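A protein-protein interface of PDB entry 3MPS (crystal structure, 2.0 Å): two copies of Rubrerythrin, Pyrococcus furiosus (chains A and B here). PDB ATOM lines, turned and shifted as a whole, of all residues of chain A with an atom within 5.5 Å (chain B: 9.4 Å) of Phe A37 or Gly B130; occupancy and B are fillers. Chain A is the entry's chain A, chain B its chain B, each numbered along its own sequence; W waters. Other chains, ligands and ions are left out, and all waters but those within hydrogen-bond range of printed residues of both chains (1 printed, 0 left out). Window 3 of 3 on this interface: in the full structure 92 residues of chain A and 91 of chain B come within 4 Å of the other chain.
The side-chain carboxylate (OE2) of Glu A35 sits at hydrogen-bond distance from the side-chain hydroxyl (OG1) of Thr B68 (2.8 Å).
The side-chain carboxylate (OD1) of Asp B132 lies within hydrogen-bond range of the backbone NH (N) of Asn A39.
The backbone carbonyl oxygen (O) of Ile B133 is in hydrogen-bond range of the side-chain amide nitrogen (ND2) of Asn A39.
The side-chain carboxylate (OD2) of Asp B132 lies within hydrogen-bond range of the backbone NH (N) of Ile A40 (3.1 Å).
The backbone nitrogen (N) of Pro A38 lies close to the side-chain carboxylate (OD1) of Asp B132 (3.1 Å).
N of Phe A37 sits at hydrogen-bond distance from O of Ala A32 (2.9 Å).
OD1 of Asn A39 lies within hydrogen-bond range of NZ of Lys A42, 3.1 Å away.
The backbone NH of Lys B67 is in hydrogen-bond range of the side-chain carboxylate of Glu B70 (3.0 Å).
The backbone carbonyl oxygen (O) of Lys B67 sits close to the side-chain amide nitrogen (ND2) of Asn B71, 3.2 Å away.
O of Lys B126 is in hydrogen-bond range of N of Glu B131.
Among the printed residues, merely in contact across the chains: Ala A32 with Thr B68 (3.4 Å), Glu A35 with Lys B67 (3.4 Å), Phe A37 with Thr B68 (3.8 Å), Phe A37 with Gly B130 (3.9 Å), Phe A37 with Glu B131 (3.8 Å), Phe A37 with Asp B132 (3.5 Å), Ile A40 with Thr B68 (3.7 Å), Ile A40 with Ala B123 (3.8 Å), Ile A40 with Ala B127 (3.7 Å) and Ile A40 with Ile B133 (3.7 Å).
No residue of chain B comes within 4 Å of Gly A36.
Gly B66 touches none of the printed residues of chain A.
Printed residues of chain A within 4 Å of Thr B68: Ala A32, Glu A35, Phe A37 and Ile A40.
Printed residues of chain A within 4 Å of Ala B123: Ile A40 (3.8 Å).
Of the printed residues of chain A, Ala B127 touches Ile A40.
Gly B130 touches just one residue of chain A: Phe A37.
Printed residues of chain A within 4 Å of Glu B131: Phe A37 (3.8 Å).
Printed residues of chain A within 4 Å of Asp B132: Phe A37, Pro A38, Asn A39 and Ile A40.
The nearest printed residue of chain A that does not touch Gly B130 is Gly A36 (6.5 Å).
The nearest printed residue of chain A that does not touch Ala B123 is Asn A39 (7.2 Å).
Of the 10 printed residues of chain A, 6 touch a printed residue of chain B.
Hydrophobic or aromatic side chains of chain A within 4 Å of the printed part of chain B: Ala A32, Phe A37, Pro A38 and Ile A40.
Along chain B the printed residues that touch a printed residue of chain A span positions 67 to 133.
Among the printed residues, 15 pairs touch across the chains.
Among the printed residues, no Asp or Glu carboxylate lies within 4 Å of a Lys or Arg side-chain nitrogen of the other chain.
No position is printed for both chains.
Water W1 lies within hydrogen-bond range of OG1 of Thr B68 (2.9 Å), ND2 of Asn B71 (3.1 Å) and N of Ala A32 (3.4 Å).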
ATOM      1  N   ALA A  32       8.693  23.920  -9.778  1.00  0.00           N
ATOM      2  CA  ALA A  32       9.840  23.358 -10.479  1.00  0.00           C
ATOM      3  C   ALA A  32      10.863  24.433 -10.864  1.00  0.00           C
ATOM      4  O   ALA A  32      12.057  24.271 -10.603  1.00  0.00           O
ATOM      5  CB  ALA A  32       9.389  22.561 -11.723  1.00  0.00           C
ATOM      6  N   GLU A  33      10.387  25.519 -11.481  1.00  0.00           N
ATOM      7  CA  GLU A  33      11.220  26.688 -11.816  1.00  0.00           C
ATOM      8  C   GLU A  33      11.955  27.254 -10.584  1.00  0.00           C
ATOM      9  O   GLU A  33      13.150  27.575 -10.639  1.00  0.00           O
ATOM     10  CB  GLU A  33      10.349  27.770 -12.473  1.00  0.00           C
ATOM     11  CG  GLU A  33      11.115  28.875 -13.231  1.00  0.00           C
ATOM     12  CD  GLU A  33      11.751  28.396 -14.545  1.00  0.00           C
ATOM     13  OE1 GLU A  33      11.175  27.515 -15.224  1.00  0.00           O
ATOM     14  OE2 GLU A  33      12.835  28.907 -14.901  1.00  0.00           O
ATOM     15  N   GLU A  35      12.671  25.580  -7.767  1.00  0.00           N
ATOM     16  CA  GLU A  35      13.625  24.600  -7.249  1.00  0.00           C
ATOM     17  C   GLU A  35      14.777  24.327  -8.224  1.00  0.00           C
ATOM     18  O   GLU A  35      15.631  23.493  -7.957  1.00  0.00           O
ATOM     19  CB  GLU A  35      12.907  23.306  -6.832  1.00  0.00           C
ATOM     20  CG  GLU A  35      11.954  23.478  -5.628  1.00  0.00           C
ATOM     21  CD  GLU A  35      11.246  22.189  -5.221  1.00  0.00           C
ATOM     22  OE1 GLU A  35      10.699  22.146  -4.099  1.00  0.00           O
ATOM     23  OE2 GLU A  35      11.230  21.221  -6.014  1.00  0.00           O
ATOM     24  N   GLY A  36      14.796  25.049  -9.343  1.00  0.00           N
ATOM     25  CA  GLY A  36      15.918  25.015 -10.293  1.00  0.00           C
ATOM     26  C   GLY A  36      15.836  23.909 -11.338  1.00  0.00           C
ATOM     27  O   GLY A  36      16.861  23.421 -11.821  1.00  0.00           O
ATOM     28  N   PHE A  37      14.617  23.517 -11.691  1.00  0.00           N
ATOM     29  CA  PHE A  37      14.392  22.509 -12.711  1.00  0.00           C
ATOM     30  C   PHE A  37      13.566  23.141 -13.843  1.00  0.00           C
ATOM     31  O   PHE A  37      12.358  22.951 -13.895  1.00  0.00           O
ATOM     32  CB  PHE A  37      13.629  21.292 -12.145  1.00  0.00           C
ATOM     33  CG  PHE A  37      14.258  20.656 -10.915  1.00  0.00           C
ATOM     34  CD1 PHE A  37      13.570  20.646  -9.699  1.00  0.00           C
ATOM     35  CD2 PHE A  37      15.512  20.047 -10.979  1.00  0.00           C
ATOM     36  CE1 PHE A  37      14.122  20.053  -8.556  1.00  0.00           C
ATOM     37  CE2 PHE A  37      16.084  19.449  -9.837  1.00  0.00           C
ATOM     38  CZ  PHE A  37      15.385  19.448  -8.627  1.00  0.00           C
ATOM     39  N   PRO A  38      14.214  23.894 -14.753  1.00  0.00           N
ATOM     40  CA  PRO A  38      13.443  24.598 -15.789  1.00  0.00           C
ATOM     41  C   PRO A  38      12.857  23.710 -16.890  1.00  0.00           C
ATOM     42  O   PRO A  38      11.826  24.057 -17.447  1.00  0.00           O
ATOM     43  CB  PRO A  38      14.476  25.547 -16.397  1.00  0.00           C
ATOM     44  CG  PRO A  38      15.775  24.820 -16.238  1.00  0.00           C
ATOM     45  CD  PRO A  38      15.661  24.165 -14.874  1.00  0.00           C
ATOM     46  N   ASN A  39      13.509  22.604 -17.237  1.00  0.00           N
ATOM     47  CA  ASN A  39      12.938  21.722 -18.256  1.00  0.00           C
ATOM     48  C   ASN A  39      11.734  20.946 -17.734  1.00  0.00           C
ATOM     49  O   ASN A  39      10.796  20.669 -18.487  1.00  0.00           O
ATOM     50  CB  ASN A  39      13.980  20.783 -18.853  1.00  0.00           C
ATOM     51  CG  ASN A  39      15.031  21.519 -19.648  1.00  0.00           C
ATOM     52  OD1 ASN A  39      14.749  22.561 -20.250  1.00  0.00           O
ATOM     53  ND2 ASN A  39      16.250  20.992 -19.651  1.00  0.00           N
ATOM     54  N   ILE A  40      11.761  20.615 -16.445  1.00  0.00           N
ATOM     55  CA  ILE A  40      10.595  20.036 -15.774  1.00  0.00           C
ATOM     56  C   ILE A  40       9.422  21.030 -15.752  1.00  0.00           C
ATOM     57  O   ILE A  40       8.274  20.642 -15.973  1.00  0.00           O
ATOM     58  CB  ILE A  40      10.946  19.503 -14.347  1.00  0.00           C
ATOM     59  CG1 ILE A  40      11.862  18.267 -14.454  1.00  0.00           C
ATOM     60  CG2 ILE A  40       9.680  19.166 -13.563  1.00  0.00           C
ATOM     61  CD1 ILE A  40      12.248  17.601 -13.114  1.00  0.00           C
ATOM     62  N   ALA A  41       9.712  22.308 -15.484  1.00  0.00           N
ATOM     63  CA  ALA A  41       8.682  23.355 -15.495  1.00  0.00           C
ATOM     64  C   ALA A  41       8.016  23.461 -16.869  1.00  0.00           C
ATOM     65  O   ALA A  41       6.790  23.504 -16.966  1.00  0.00           O
ATOM     66  CB  ALA A  41       9.275  24.698 -15.082  1.00  0.00           C
ATOM     67  N   LYS A  42       8.841  23.473 -17.919  1.00  0.00           N
ATOM     68  CA  LYS A  42       8.372  23.461 -19.316  1.00  0.00           C
ATOM     69  C   LYS A  42       7.499  22.238 -19.627  1.00  0.00           C
ATOM     70  O   LYS A  42       6.476  22.366 -20.297  1.00  0.00           O
ATOM     71  CB  LYS A  42       9.570  23.532 -20.272  1.00  0.00           C
ATOM     72  CG  LYS A  42       9.222  23.671 -21.750  1.00  0.00           C
ATOM     73  CD  LYS A  42      10.485  23.623 -22.632  1.00  0.00           C
ATOM     74  CE  LYS A  42      11.364  22.408 -22.315  1.00  0.00           C
ATOM     75  NZ  LYS A  42      12.806  22.675 -22.612  1.00  0.00           N
ATOM     76  N   GLY B  66       4.229  20.462  -2.599  1.00  0.00           N
ATOM     77  CA  GLY B  66       5.469  19.990  -1.988  1.00  0.00           C
ATOM     78  C   GLY B  66       6.613  20.164  -2.967  1.00  0.00           C
ATOM     79  O   GLY B  66       6.582  21.057  -3.815  1.00  0.00           O
ATOM     80  N   LYS B  67       7.612  19.297  -2.856  1.00  0.00           N
ATOM     81  CA  LYS B  67       8.770  19.330  -3.730  1.00  0.00           C
ATOM     82  C   LYS B  67       8.407  18.731  -5.098  1.00  0.00           C
ATOM     83  O   LYS B  67       7.455  17.950  -5.216  1.00  0.00           O
ATOM     84  CB  LYS B  67       9.938  18.580  -3.075  1.00  0.00           C
ATOM     85  CG  LYS B  67      10.258  19.080  -1.675  1.00  0.00           C
ATOM     86  CD  LYS B  67      10.542  17.925  -0.738  1.00  0.00           C
ATOM     87  CE  LYS B  67      11.962  17.892  -0.291  1.00  0.00           C
ATOM     88  NZ  LYS B  67      12.110  18.582   1.018  1.00  0.00           N
ATOM     89  N   THR B  68       9.167  19.104  -6.121  1.00  0.00           N
ATOM     90  CA  THR B  68       8.952  18.621  -7.502  1.00  0.00           C
ATOM     91  C   THR B  68       8.793  17.087  -7.669  1.00  0.00           C
ATOM     92  O   THR B  68       7.897  16.642  -8.385  1.00  0.00           O
ATOM     93  CB  THR B  68      10.054  19.158  -8.446  1.00  0.00           C
ATOM     94  OG1 THR B  68      10.012  20.587  -8.439  1.00  0.00           O
ATOM     95  CG2 THR B  68       9.854  18.669  -9.862  1.00  0.00           C
ATOM     96  N   PRO B  69       9.650  16.276  -7.006  1.00  0.00           N
ATOM     97  CA  PRO B  69       9.478  14.844  -7.180  1.00  0.00           C
ATOM     98  C   PRO B  69       8.155  14.347  -6.590  1.00  0.00           C
ATOM     99  O   PRO B  69       7.565  13.395  -7.102  1.00  0.00           O
ATOM    100  CB  PRO B  69      10.678  14.246  -6.420  1.00  0.00           C
ATOM    101  CG  PRO B  69      11.624  15.350  -6.239  1.00  0.00           C
ATOM    102  CD  PRO B  69      10.789  16.573  -6.114  1.00  0.00           C
ATOM    103  N   GLU B  70       7.703  15.035  -5.541  1.00  0.00           N
ATOM    104  CA  GLU B  70       6.467  14.736  -4.838  1.00  0.00           C
ATOM    105  C   GLU B  70       5.274  15.192  -5.674  1.00  0.00           C
ATOM    106  O   GLU B  70       4.265  14.496  -5.752  1.00  0.00           O
ATOM    107  CB  GLU B  70       6.486  15.404  -3.464  1.00  0.00           C
ATOM    108  CG  GLU B  70       7.708  14.962  -2.636  1.00  0.00           C
ATOM    109  CD  GLU B  70       7.855  15.679  -1.309  1.00  0.00           C
ATOM    110  OE1 GLU B  70       7.317  16.803  -1.143  1.00  0.00           O
ATOM    111  OE2 GLU B  70       8.526  15.099  -0.427  1.00  0.00           O
ATOM    112  N   ASN B  71       5.416  16.339  -6.326  1.00  0.00           N
ATOM    113  CA  ASN B  71       4.400  16.837  -7.255  1.00  0.00           C
ATOM    114  C   ASN B  71       4.307  15.965  -8.515  1.00  0.00           C
ATOM    115  O   ASN B  71       3.217  15.763  -9.068  1.00  0.00           O
ATOM    116  CB  ASN B  71       4.701  18.287  -7.637  1.00  0.00           C
ATOM    117  CG  ASN B  71       4.830  19.203  -6.425  1.00  0.00           C
ATOM    118  OD1 ASN B  71       4.175  19.000  -5.394  1.00  0.00           O
ATOM    119  ND2 ASN B  71       5.669  20.228  -6.551  1.00  0.00           N
ATOM    120  N   LEU B  72       5.451  15.444  -8.957  1.00  0.00           N
ATOM    121  CA  LEU B  72       5.477  14.550 -10.106  1.00  0.00           C
ATOM    122  C   LEU B  72       4.764  13.236  -9.818  1.00  0.00           C
ATOM    123  O   LEU B  72       4.094  12.705 -10.688  1.00  0.00           O
ATOM    124  CB  LEU B  72       6.913  14.300 -10.588  1.00  0.00           C
ATOM    125  CG  LEU B  72       7.508  15.458 -11.391  1.00  0.00           C
ATOM    126  CD1 LEU B  72       9.026  15.370 -11.349  1.00  0.00           C
ATOM    127  CD2 LEU B  72       6.980  15.445 -12.810  1.00  0.00           C
ATOM    128  N   ALA B 123      10.746  12.074 -15.567  1.00  0.00           N
ATOM    129  CA  ALA B 123      11.054  13.339 -14.897  1.00  0.00           C
ATOM    130  C   ALA B 123      11.332  13.146 -13.400  1.00  0.00           C
ATOM    131  O   ALA B 123      12.182  13.837 -12.815  1.00  0.00           O
ATOM    132  CB  ALA B 123       9.940  14.342 -15.109  1.00  0.00           C
ATOM    133  N   LYS B 124      10.622  12.205 -12.784  1.00  0.00           N
ATOM    134  CA  LYS B 124      10.774  11.975 -11.357  1.00  0.00           C
ATOM    135  C   LYS B 124      12.118  11.309 -11.039  1.00  0.00           C
ATOM    136  O   LYS B 124      12.777  11.718 -10.100  1.00  0.00           O
ATOM    137  CB  LYS B 124       9.594  11.177 -10.777  1.00  0.00           C
ATOM    138  CG  LYS B 124       9.531  11.188  -9.252  1.00  0.00           C
ATOM    139  CD  LYS B 124       8.446  10.254  -8.730  1.00  0.00           C
ATOM    140  CE  LYS B 124       8.704   9.864  -7.279  1.00  0.00           C
ATOM    141  NZ  LYS B 124       7.668   8.917  -6.733  1.00  0.00           N
ATOM    142  N   GLU B 125      12.526  10.311 -11.827  1.00  0.00           N
ATOM    143  CA  GLU B 125      13.830   9.665 -11.605  1.00  0.00           C
ATOM    144  C   GLU B 125      15.018  10.648 -11.685  1.00  0.00           C
ATOM    145  O   GLU B 125      16.036  10.451 -11.021  1.00  0.00           O
ATOM    146  CB  GLU B 125      14.047   8.417 -12.485  1.00  0.00           C
ATOM    147  CG  GLU B 125      13.980   8.573 -14.008  1.00  0.00           C
ATOM    148  CD  GLU B 125      14.214   7.251 -14.759  1.00  0.00           C
ATOM    149  OE1 GLU B 125      13.562   7.030 -15.815  1.00  0.00           O
ATOM    150  OE2 GLU B 125      15.046   6.423 -14.293  1.00  0.00           O
ATOM    151  N   LYS B 126      14.866  11.708 -12.473  1.00  0.00           N
ATOM    152  CA  LYS B 126      15.909  12.728 -12.580  1.00  0.00           C
ATOM    153  C   LYS B 126      15.855  13.668 -11.382  1.00  0.00           C
ATOM    154  O   LYS B 126      16.860  13.859 -10.699  1.00  0.00           O
ATOM    155  CB  LYS B 126      15.798  13.492 -13.904  1.00  0.00           C
ATOM    156  CG  LYS B 126      16.047  12.613 -15.125  1.00  0.00           C
ATOM    157  CD  LYS B 126      17.537  12.482 -15.444  1.00  0.00           C
ATOM    158  CE  LYS B 126      17.819  11.272 -16.331  1.00  0.00           C
ATOM    159  NZ  LYS B 126      19.146  11.364 -17.038  1.00  0.00           N
ATOM    160  N   ALA B 127      14.673  14.217 -11.111  1.00  0.00           N
ATOM    161  CA  ALA B 127      14.475  15.144  -9.990  1.00  0.00           C
ATOM    162  C   ALA B 127      14.799  14.509  -8.630  1.00  0.00           C
ATOM    163  O   ALA B 127      15.326  15.173  -7.740  1.00  0.00           O
ATOM    164  CB  ALA B 127      13.073  15.697 -10.004  1.00  0.00           C
ATOM    165  N   GLU B 128      14.463  13.228  -8.474  1.00  0.00           N
ATOM    166  CA  GLU B 128      14.937  12.435  -7.330  1.00  0.00           C
ATOM    167  C   GLU B 128      16.408  12.729  -7.059  1.00  0.00           C
ATOM    168  O   GLU B 128      16.768  13.201  -5.973  1.00  0.00           O
ATOM    169  CB  GLU B 128      14.757  10.928  -7.577  1.00  0.00           C
ATOM    170  CG  GLU B 128      13.332  10.406  -7.366  1.00  0.00           C
ATOM    171  CD  GLU B 128      12.795  10.664  -5.968  1.00  0.00           C
ATOM    172  OE1 GLU B 128      13.330  11.564  -5.269  1.00  0.00           O
ATOM    173  OE2 GLU B 128      11.835   9.968  -5.574  1.00  0.00           O
ATOM    174  N   LYS B 129      17.235  12.487  -8.077  1.00  0.00           N
ATOM    175  CA  LYS B 129      18.684  12.578  -7.962  1.00  0.00           C
ATOM    176  C   LYS B 129      19.231  14.001  -8.116  1.00  0.00           C
ATOM    177  O   LYS B 129      20.437  14.193  -8.217  1.00  0.00           O
ATOM    178  CB  LYS B 129      19.357  11.607  -8.946  1.00  0.00           C
ATOM    179  CG  LYS B 129      19.305  10.145  -8.501  1.00  0.00           C
ATOM    180  CD  LYS B 129      20.391   9.303  -9.176  1.00  0.00           C
ATOM    181  CE  LYS B 129      20.649   7.991  -8.434  1.00  0.00           C
ATOM    182  NZ  LYS B 129      19.563   6.987  -8.680  1.00  0.00           N
ATOM    183  N   GLY B 130      18.337  14.986  -8.125  1.00  0.00           N
ATOM    184  CA  GLY B 130      18.706  16.407  -8.074  1.00  0.00           C
ATOM    185  C   GLY B 130      19.021  16.988  -9.436  1.00  0.00           C
ATOM    186  O   GLY B 130      19.682  18.028  -9.548  1.00  0.00           O
ATOM    187  N   GLU B 131      18.536  16.306 -10.468  1.00  0.00           N
ATOM    188  CA  GLU B 131      18.834  16.650 -11.852  1.00  0.00           C
ATOM    189  C   GLU B 131      17.569  17.029 -12.605  1.00  0.00           C
ATOM    190  O   GLU B 131      16.469  16.562 -12.277  1.00  0.00           O
ATOM    191  CB  GLU B 131      19.533  15.485 -12.554  1.00  0.00           C
ATOM    192  CG  GLU B 131      20.829  15.049 -11.874  1.00  0.00           C
ATOM    193  CD  GLU B 131      21.442  13.817 -12.498  1.00  0.00           C
ATOM    194  OE1 GLU B 131      21.177  13.548 -13.690  1.00  0.00           O
ATOM    195  OE2 GLU B 131      22.204  13.123 -11.794  1.00  0.00           O
ATOM    196  N   ASP B 132      17.739  17.887 -13.602  1.00  0.00           N
ATOM    197  CA  ASP B 132      16.641  18.308 -14.454  1.00  0.00           C
ATOM    198  C   ASP B 132      16.519  17.289 -15.568  1.00  0.00           C
ATOM    199  O   ASP B 132      17.377  16.411 -15.711  1.00  0.00           O
ATOM    200  CB  ASP B 132      16.905  19.707 -15.023  1.00  0.00           C
ATOM    201  CG  ASP B 132      15.633  20.388 -15.532  1.00  0.00           C
ATOM    202  OD1 ASP B 132      15.739  21.493 -16.095  1.00  0.00           O
ATOM    203  OD2 ASP B 132      14.530  19.819 -15.385  1.00  0.00           O
ATOM    204  N   ILE B 133      15.449  17.393 -16.344  1.00  0.00           N
ATOM    205  CA  ILE B 133      15.302  16.565 -17.532  1.00  0.00           C
ATOM    206  C   ILE B 133      16.011  17.229 -18.721  1.00  0.00           C
ATOM    207  O   ILE B 133      16.214  18.453 -18.733  1.00  0.00           O
ATOM    208  CB  ILE B 133      13.822  16.239 -17.831  1.00  0.00           C
ATOM    209  CG1 ILE B 133      12.998  17.524 -17.977  1.00  0.00           C
ATOM    210  CG2 ILE B 133      13.256  15.312 -16.740  1.00  0.00           C
ATOM    211  CD1 ILE B 133      11.544  17.310 -18.302  1.00  0.00           C
ATOM    212  N   GLU B 134      16.402  16.415 -19.698  1.00  0.00           N
ATOM    213  CA  GLU B 134      17.190  16.883 -20.846  1.00  0.00           C
ATOM    214  C   GLU B 134      16.325  17.336 -22.030  1.00  0.00           C
ATOM    215  O   GLU B 134      16.820  18.008 -22.944  1.00  0.00           O
ATOM    216  CB  GLU B 134      18.151  15.789 -21.320  1.00  0.00           C
ATOM    217  CG  GLU B 134      19.382  15.543 -20.447  1.00  0.00           C
ATOM    218  CD  GLU B 134      20.371  14.568 -21.094  1.00  0.00           C
ATOM    219  OE1 GLU B 134      21.260  14.042 -20.380  1.00  0.00           O
ATOM    220  OE2 GLU B 134      20.261  14.318 -22.319  1.00  0.00           O
HETATM  221  O   HOH W   1       7.206  20.963  -9.098  1.00  0.00           O
